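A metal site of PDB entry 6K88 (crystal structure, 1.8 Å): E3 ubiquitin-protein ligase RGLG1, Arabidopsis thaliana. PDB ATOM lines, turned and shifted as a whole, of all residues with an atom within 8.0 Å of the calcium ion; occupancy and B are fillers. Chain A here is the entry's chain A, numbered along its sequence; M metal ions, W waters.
N of Thr 136 sits at hydrogen-bond distance from OG1 of Thr 168 (2.8 Å). The side-chain carboxylate (OD2) of Asp 164 sits close to the side-chain hydroxyl (OG) of Ser 44 (2.5 Å). The backbone carbonyl oxygen (O) of Ser 44 sits at hydrogen-bond distance from the side-chain hydroxyl (OG1) of Thr 48, at 3.0 Å. N of Thr 42 is in hydrogen-bond range of OD1 of Asp 40 (2.8 Å). ND2 of Asn 45 sits at hydrogen-bond distance from O of Thr 42, 2.9 Å away. N of Gln 166 lies within hydrogen-bond range of OD1 of Asp 164, 3.0 Å away.
Four residues have an atom within 4 Å of the calcium ion: Thr 42, Ser 44, Thr 136 and Gln 166. The nearest printed residue that does not touch the calcium ion is Asp 164 (4.1 Å).
The side-chain hydroxyl (OG1) of Thr 136 is bound to the calcium ion. The calcium ion is bound by water W2, 2.4 Å away. Water W1 binds the calcium ion (2.4 Å). OG of Ser 44 binds the calcium ion, 2.5 Å away. OG1 of Thr 42 binds the calcium ion, at 2.5 Å. The backbone carbonyl oxygen (O) of Gln 166 is bound to the calcium ion (2.6 Å). The calcium ion has six donor atoms within binding distance.
Water W2 lies within hydrogen-bond range of the side-chain carboxylate (OD1) of Asp 164 (2.4 Å) and the side-chain carboxylate (OD2) of Asp 40 (2.7 Å).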
ATOM      1  N   ASP A  40     -18.979  21.514  27.641  1.00  0.00           N
ATOM      2  CA  ASP A  40     -20.039  20.507  27.593  1.00  0.00           C
ATOM      3  C   ASP A  40     -19.530  19.169  28.124  1.00  0.00           C
ATOM      4  O   ASP A  40     -18.646  18.553  27.536  1.00  0.00           O
ATOM      5  CB  ASP A  40     -20.529  20.393  26.134  1.00  0.00           C
ATOM      6  CG  ASP A  40     -21.701  19.432  25.950  1.00  0.00           C
ATOM      7  OD1 ASP A  40     -21.685  18.303  26.488  1.00  0.00           O
ATOM      8  OD2 ASP A  40     -22.638  19.830  25.213  1.00  0.00           O
ATOM      9  N   PHE A  41     -20.118  18.707  29.225  1.00  0.00           N
ATOM     10  CA  PHE A  41     -19.797  17.414  29.809  1.00  0.00           C
ATOM     11  C   PHE A  41     -20.991  16.437  29.747  1.00  0.00           C
ATOM     12  O   PHE A  41     -21.233  15.676  30.698  1.00  0.00           O
ATOM     13  CB  PHE A  41     -19.342  17.573  31.260  1.00  0.00           C
ATOM     14  CG  PHE A  41     -17.997  18.231  31.399  1.00  0.00           C
ATOM     15  CD1 PHE A  41     -16.842  17.580  30.999  1.00  0.00           C
ATOM     16  CD2 PHE A  41     -17.887  19.512  31.932  1.00  0.00           C
ATOM     17  CE1 PHE A  41     -15.594  18.193  31.126  1.00  0.00           C
ATOM     18  CE2 PHE A  41     -16.667  20.118  32.060  1.00  0.00           C
ATOM     19  CZ  PHE A  41     -15.521  19.470  31.656  1.00  0.00           C
ATOM     20  N   THR A  42     -21.734  16.463  28.636  1.00  0.00           N
ATOM     21  CA  THR A  42     -22.868  15.555  28.532  1.00  0.00           C
ATOM     22  C   THR A  42     -22.444  14.231  27.938  1.00  0.00           C
ATOM     23  O   THR A  42     -21.353  14.100  27.356  1.00  0.00           O
ATOM     24  CB  THR A  42     -24.033  16.177  27.715  1.00  0.00           C
ATOM     25  OG1 THR A  42     -23.617  16.430  26.372  1.00  0.00           O
ATOM     26  CG2 THR A  42     -24.474  17.491  28.371  1.00  0.00           C
ATOM     27  N   LYS A  43     -23.309  13.226  28.102  1.00  0.00           N
ATOM     28  CA  LYS A  43     -22.979  11.857  27.742  1.00  0.00           C
ATOM     29  C   LYS A  43     -22.813  11.632  26.220  1.00  0.00           C
ATOM     30  O   LYS A  43     -22.158  10.666  25.801  1.00  0.00           O
ATOM     31  CB  LYS A  43     -24.051  10.911  28.308  1.00  0.00           C
ATOM     32  CG  LYS A  43     -23.650   9.427  28.338  1.00  0.00           C
ATOM     33  CD  LYS A  43     -24.731   8.600  29.032  1.00  0.00           C
ATOM     34  CE  LYS A  43     -24.412   7.109  28.938  1.00  0.00           C
ATOM     35  NZ  LYS A  43     -23.079   6.811  29.534  1.00  0.00           N
ATOM     36  N   SER A  44     -23.381  12.508  25.400  1.00  0.00           N
ATOM     37  CA  SER A  44     -23.231  12.339  23.948  1.00  0.00           C
ATOM     38  C   SER A  44     -21.764  12.424  23.493  1.00  0.00           C
ATOM     39  O   SER A  44     -21.406  11.940  22.416  1.00  0.00           O
ATOM     40  CB  SER A  44     -24.066  13.358  23.170  1.00  0.00           C
ATOM     41  OG  SER A  44     -23.606  14.697  23.336  1.00  0.00           O
ATOM     42  N   ASN A  45     -20.912  13.030  24.325  1.00  0.00           N
ATOM     43  CA  ASN A  45     -19.495  13.091  23.993  1.00  0.00           C
ATOM     44  C   ASN A  45     -18.886  11.694  23.898  1.00  0.00           C
ATOM     45  O   ASN A  45     -17.854  11.510  23.257  1.00  0.00           O
ATOM     46  CB  ASN A  45     -18.741  13.929  25.037  1.00  0.00           C
ATOM     47  CG  ASN A  45     -19.017  15.428  24.889  1.00  0.00           C
ATOM     48  OD1 ASN A  45     -18.559  16.051  23.943  1.00  0.00           O
ATOM     49  ND2 ASN A  45     -19.758  16.007  25.832  1.00  0.00           N
ATOM     50  N   GLU A  46     -19.555  10.704  24.489  1.00  0.00           N
ATOM     51  CA  GLU A  46     -19.090   9.321  24.389  1.00  0.00           C
ATOM     52  C   GLU A  46     -19.196   8.739  22.988  1.00  0.00           C
ATOM     53  O   GLU A  46     -18.480   7.777  22.657  1.00  0.00           O
ATOM     54  CB  GLU A  46     -19.855   8.410  25.363  1.00  0.00           C
ATOM     55  CG  GLU A  46     -19.538   8.692  26.828  1.00  0.00           C
ATOM     56  CD  GLU A  46     -20.404   7.880  27.789  1.00  0.00           C
ATOM     57  OE1 GLU A  46     -21.226   7.041  27.341  1.00  0.00           O
ATOM     58  OE2 GLU A  46     -20.252   8.105  29.019  1.00  0.00           O
ATOM     59  N   TRP A  47     -20.075   9.286  22.161  1.00  0.00           N
ATOM     60  CA  TRP A  47     -20.209   8.753  20.798  1.00  0.00           C
ATOM     61  C   TRP A  47     -19.981   9.759  19.668  1.00  0.00           C
ATOM     62  O   TRP A  47     -19.860   9.353  18.512  1.00  0.00           O
ATOM     63  CB  TRP A  47     -21.606   8.096  20.616  1.00  0.00           C
ATOM     64  CG  TRP A  47     -22.811   8.940  20.921  1.00  0.00           C
ATOM     65  CD1 TRP A  47     -23.522   8.966  22.095  1.00  0.00           C
ATOM     66  CD2 TRP A  47     -23.486   9.851  20.030  1.00  0.00           C
ATOM     67  NE1 TRP A  47     -24.564   9.854  21.991  1.00  0.00           N
ATOM     68  CE2 TRP A  47     -24.572  10.413  20.737  1.00  0.00           C
ATOM     69  CE3 TRP A  47     -23.254  10.260  18.710  1.00  0.00           C
ATOM     70  CZ2 TRP A  47     -25.439  11.351  20.175  1.00  0.00           C
ATOM     71  CZ3 TRP A  47     -24.130  11.203  18.145  1.00  0.00           C
ATOM     72  CH2 TRP A  47     -25.202  11.742  18.879  1.00  0.00           C
ATOM     73  N   THR A  48     -19.897  11.059  19.965  1.00  0.00           N
ATOM     74  CA  THR A  48     -19.695  12.029  18.887  1.00  0.00           C
ATOM     75  C   THR A  48     -18.237  12.091  18.398  1.00  0.00           C
ATOM     76  O   THR A  48     -17.902  12.918  17.550  1.00  0.00           O
ATOM     77  CB  THR A  48     -20.130  13.460  19.314  1.00  0.00           C
ATOM     78  OG1 THR A  48     -19.704  13.711  20.650  1.00  0.00           O
ATOM     79  CG2 THR A  48     -21.632  13.614  19.230  1.00  0.00           C
ATOM     80  N   TYR A  68     -11.366  18.386  23.083  1.00  0.00           N
ATOM     81  CA  TYR A  68     -11.603  19.494  24.015  1.00  0.00           C
ATOM     82  C   TYR A  68     -10.299  20.159  24.435  1.00  0.00           C
ATOM     83  O   TYR A  68     -10.199  21.388  24.473  1.00  0.00           O
ATOM     84  CB  TYR A  68     -12.355  19.021  25.273  1.00  0.00           C
ATOM     85  CG  TYR A  68     -13.831  18.895  25.017  1.00  0.00           C
ATOM     86  CD1 TYR A  68     -14.367  17.718  24.526  1.00  0.00           C
ATOM     87  CD2 TYR A  68     -14.700  19.972  25.248  1.00  0.00           C
ATOM     88  CE1 TYR A  68     -15.713  17.599  24.273  1.00  0.00           C
ATOM     89  CE2 TYR A  68     -16.058  19.869  24.985  1.00  0.00           C
ATOM     90  CZ  TYR A  68     -16.550  18.668  24.502  1.00  0.00           C
ATOM     91  OH  TYR A  68     -17.890  18.527  24.239  1.00  0.00           O
ATOM     92  N   PHE A  93     -20.845  22.027  32.313  1.00  0.00           N
ATOM     93  CA  PHE A  93     -22.272  21.752  32.429  1.00  0.00           C
ATOM     94  C   PHE A  93     -22.625  20.390  31.827  1.00  0.00           C
ATOM     95  O   PHE A  93     -21.916  19.904  30.952  1.00  0.00           O
ATOM     96  CB  PHE A  93     -23.099  22.850  31.746  1.00  0.00           C
ATOM     97  CG  PHE A  93     -22.810  23.023  30.280  1.00  0.00           C
ATOM     98  CD1 PHE A  93     -23.484  22.248  29.339  1.00  0.00           C
ATOM     99  CD2 PHE A  93     -21.885  23.952  29.854  1.00  0.00           C
ATOM    100  CE1 PHE A  93     -23.226  22.407  27.993  1.00  0.00           C
ATOM    101  CE2 PHE A  93     -21.612  24.111  28.498  1.00  0.00           C
ATOM    102  CZ  PHE A  93     -22.287  23.340  27.566  1.00  0.00           C
ATOM    103  N   GLY A  94     -23.690  19.777  32.318  1.00  0.00           N
ATOM    104  CA  GLY A  94     -24.197  18.569  31.721  1.00  0.00           C
ATOM    105  C   GLY A  94     -23.722  17.284  32.368  1.00  0.00           C
ATOM    106  O   GLY A  94     -24.102  16.208  31.922  1.00  0.00           O
ATOM    107  N   ALA A 133     -23.480  13.234  31.727  1.00  0.00           N
ATOM    108  CA  ALA A 133     -24.919  13.004  31.839  1.00  0.00           C
ATOM    109  C   ALA A 133     -25.700  13.896  30.898  1.00  0.00           C
ATOM    110  O   ALA A 133     -25.368  14.014  29.725  1.00  0.00           O
ATOM    111  CB  ALA A 133     -25.365  13.203  33.301  1.00  0.00           C
ATOM    112  N   GLY A 134     -26.746  14.533  31.416  1.00  0.00           N
ATOM    113  CA  GLY A 134     -27.659  15.276  30.576  1.00  0.00           C
ATOM    114  C   GLY A 134     -28.950  15.578  31.321  1.00  0.00           C
ATOM    115  O   GLY A 134     -29.023  15.326  32.515  1.00  0.00           O
ATOM    116  N   PRO A 135     -29.964  16.119  30.619  1.00  0.00           N
ATOM    117  CA  PRO A 135     -30.010  16.435  29.185  1.00  0.00           C
ATOM    118  C   PRO A 135     -29.071  17.583  28.855  1.00  0.00           C
ATOM    119  O   PRO A 135     -28.478  18.149  29.789  1.00  0.00           O
ATOM    120  CB  PRO A 135     -31.472  16.853  28.955  1.00  0.00           C
ATOM    121  CG  PRO A 135     -32.230  16.428  30.197  1.00  0.00           C
ATOM    122  CD  PRO A 135     -31.219  16.472  31.305  1.00  0.00           C
ATOM    123  N   THR A 136     -28.959  17.924  27.581  1.00  0.00           N
ATOM    124  CA  THR A 136     -28.053  18.970  27.130  1.00  0.00           C
ATOM    125  C   THR A 136     -28.794  20.285  26.824  1.00  0.00           C
ATOM    126  O   THR A 136     -29.648  20.302  25.946  1.00  0.00           O
ATOM    127  CB  THR A 136     -27.296  18.543  25.857  1.00  0.00           C
ATOM    128  OG1 THR A 136     -26.696  17.252  26.048  1.00  0.00           O
ATOM    129  CG2 THR A 136     -26.239  19.609  25.463  1.00  0.00           C
ATOM    130  N   SER A 137     -28.452  21.358  27.533  1.00  0.00           N
ATOM    131  CA  SER A 137     -28.970  22.688  27.215  1.00  0.00           C
ATOM    132  C   SER A 137     -27.862  23.741  27.371  1.00  0.00           C
ATOM    133  O   SER A 137     -26.989  23.576  28.208  1.00  0.00           O
ATOM    134  CB  SER A 137     -30.136  23.054  28.128  1.00  0.00           C
ATOM    135  OG  SER A 137     -30.556  24.381  27.883  1.00  0.00           O
ATOM    136  N   PHE A 138     -27.919  24.814  26.581  1.00  0.00           N
ATOM    137  CA  PHE A 138     -26.980  25.920  26.752  1.00  0.00           C
ATOM    138  C   PHE A 138     -27.575  27.037  27.593  1.00  0.00           C
ATOM    139  O   PHE A 138     -26.917  28.025  27.862  1.00  0.00           O
ATOM    140  CB  PHE A 138     -26.523  26.516  25.404  1.00  0.00           C
ATOM    141  CG  PHE A 138     -25.785  25.540  24.514  1.00  0.00           C
ATOM    142  CD1 PHE A 138     -25.152  24.436  25.032  1.00  0.00           C
ATOM    143  CD2 PHE A 138     -25.749  25.753  23.139  1.00  0.00           C
ATOM    144  CE1 PHE A 138     -24.490  23.549  24.197  1.00  0.00           C
ATOM    145  CE2 PHE A 138     -25.079  24.887  22.305  1.00  0.00           C
ATOM    146  CZ  PHE A 138     -24.450  23.775  22.827  1.00  0.00           C
ATOM    147  N   ALA A 163     -18.228  22.339  22.688  1.00  0.00           N
ATOM    148  CA  ALA A 163     -19.313  21.353  22.753  1.00  0.00           C
ATOM    149  C   ALA A 163     -19.373  20.488  21.498  1.00  0.00           C
ATOM    150  O   ALA A 163     -18.829  20.854  20.457  1.00  0.00           O
ATOM    151  CB  ALA A 163     -20.658  22.059  22.931  1.00  0.00           C
ATOM    152  N   ASP A 164     -20.079  19.360  21.594  1.00  0.00           N
ATOM    153  CA  ASP A 164     -20.211  18.452  20.470  1.00  0.00           C
ATOM    154  C   ASP A 164     -21.465  18.743  19.645  1.00  0.00           C
ATOM    155  O   ASP A 164     -21.780  18.022  18.689  1.00  0.00           O
ATOM    156  CB  ASP A 164     -20.187  16.981  20.950  1.00  0.00           C
ATOM    157  CG  ASP A 164     -21.475  16.545  21.668  1.00  0.00           C
ATOM    158  OD1 ASP A 164     -22.388  17.370  21.957  1.00  0.00           O
ATOM    159  OD2 ASP A 164     -21.562  15.326  21.987  1.00  0.00           O
ATOM    160  N   GLY A 165     -22.190  19.790  20.007  1.00  0.00           N
ATOM    161  CA  GLY A 165     -23.298  20.241  19.203  1.00  0.00           C
ATOM    162  C   GLY A 165     -24.618  19.550  19.482  1.00  0.00           C
ATOM    163  O   GLY A 165     -25.656  19.956  18.947  1.00  0.00           O
ATOM    164  N   GLN A 166     -24.603  18.526  20.343  1.00  0.00           N
ATOM    165  CA  GLN A 166     -25.807  17.707  20.514  1.00  0.00           C
ATOM    166  C   GLN A 166     -26.698  18.154  21.676  1.00  0.00           C
ATOM    167  O   GLN A 166     -26.697  17.559  22.764  1.00  0.00           O
ATOM    168  CB  GLN A 166     -25.417  16.242  20.648  1.00  0.00           C
ATOM    169  CG  GLN A 166     -24.517  15.760  19.508  1.00  0.00           C
ATOM    170  CD  GLN A 166     -25.030  16.145  18.119  1.00  0.00           C
ATOM    171  OE1 GLN A 166     -26.124  15.724  17.716  1.00  0.00           O
ATOM    172  NE2 GLN A 166     -24.250  16.944  17.386  1.00  0.00           N
ATOM    173  N   VAL A 167     -27.458  19.207  21.413  1.00  0.00           N
ATOM    174  CA  VAL A 167     -28.441  19.731  22.342  1.00  0.00           C
ATOM    175  C   VAL A 167     -29.632  18.767  22.285  1.00  0.00           C
ATOM    176  O   VAL A 167     -29.922  18.236  21.223  1.00  0.00           O
ATOM    177  CB  VAL A 167     -28.853  21.175  21.949  1.00  0.00           C
ATOM    178  CG1 VAL A 167     -30.064  21.635  22.732  1.00  0.00           C
ATOM    179  CG2 VAL A 167     -27.681  22.134  22.158  1.00  0.00           C
ATOM    180  N   THR A 168     -30.279  18.538  23.418  1.00  0.00           N
ATOM    181  CA  THR A 168     -31.374  17.557  23.455  1.00  0.00           C
ATOM    182  C   THR A 168     -32.516  17.938  22.512  1.00  0.00           C
ATOM    183  O   THR A 168     -32.994  19.076  22.543  1.00  0.00           O
ATOM    184  CB  THR A 168     -31.940  17.401  24.871  1.00  0.00           C
ATOM    185  OG1 THR A 168     -30.892  16.962  25.752  1.00  0.00           O
ATOM    186  CG2 THR A 168     -33.091  16.382  24.887  1.00  0.00           C
HETATM  187 CA    CA M   1     -25.339  16.119  24.524  1.00  0.00          CA
HETATM  188  O   HOH W   1     -27.155  14.952  23.389  1.00  0.00           O
HETATM  189  O   HOH W   2     -23.861  17.851  23.841  1.00  0.00           O
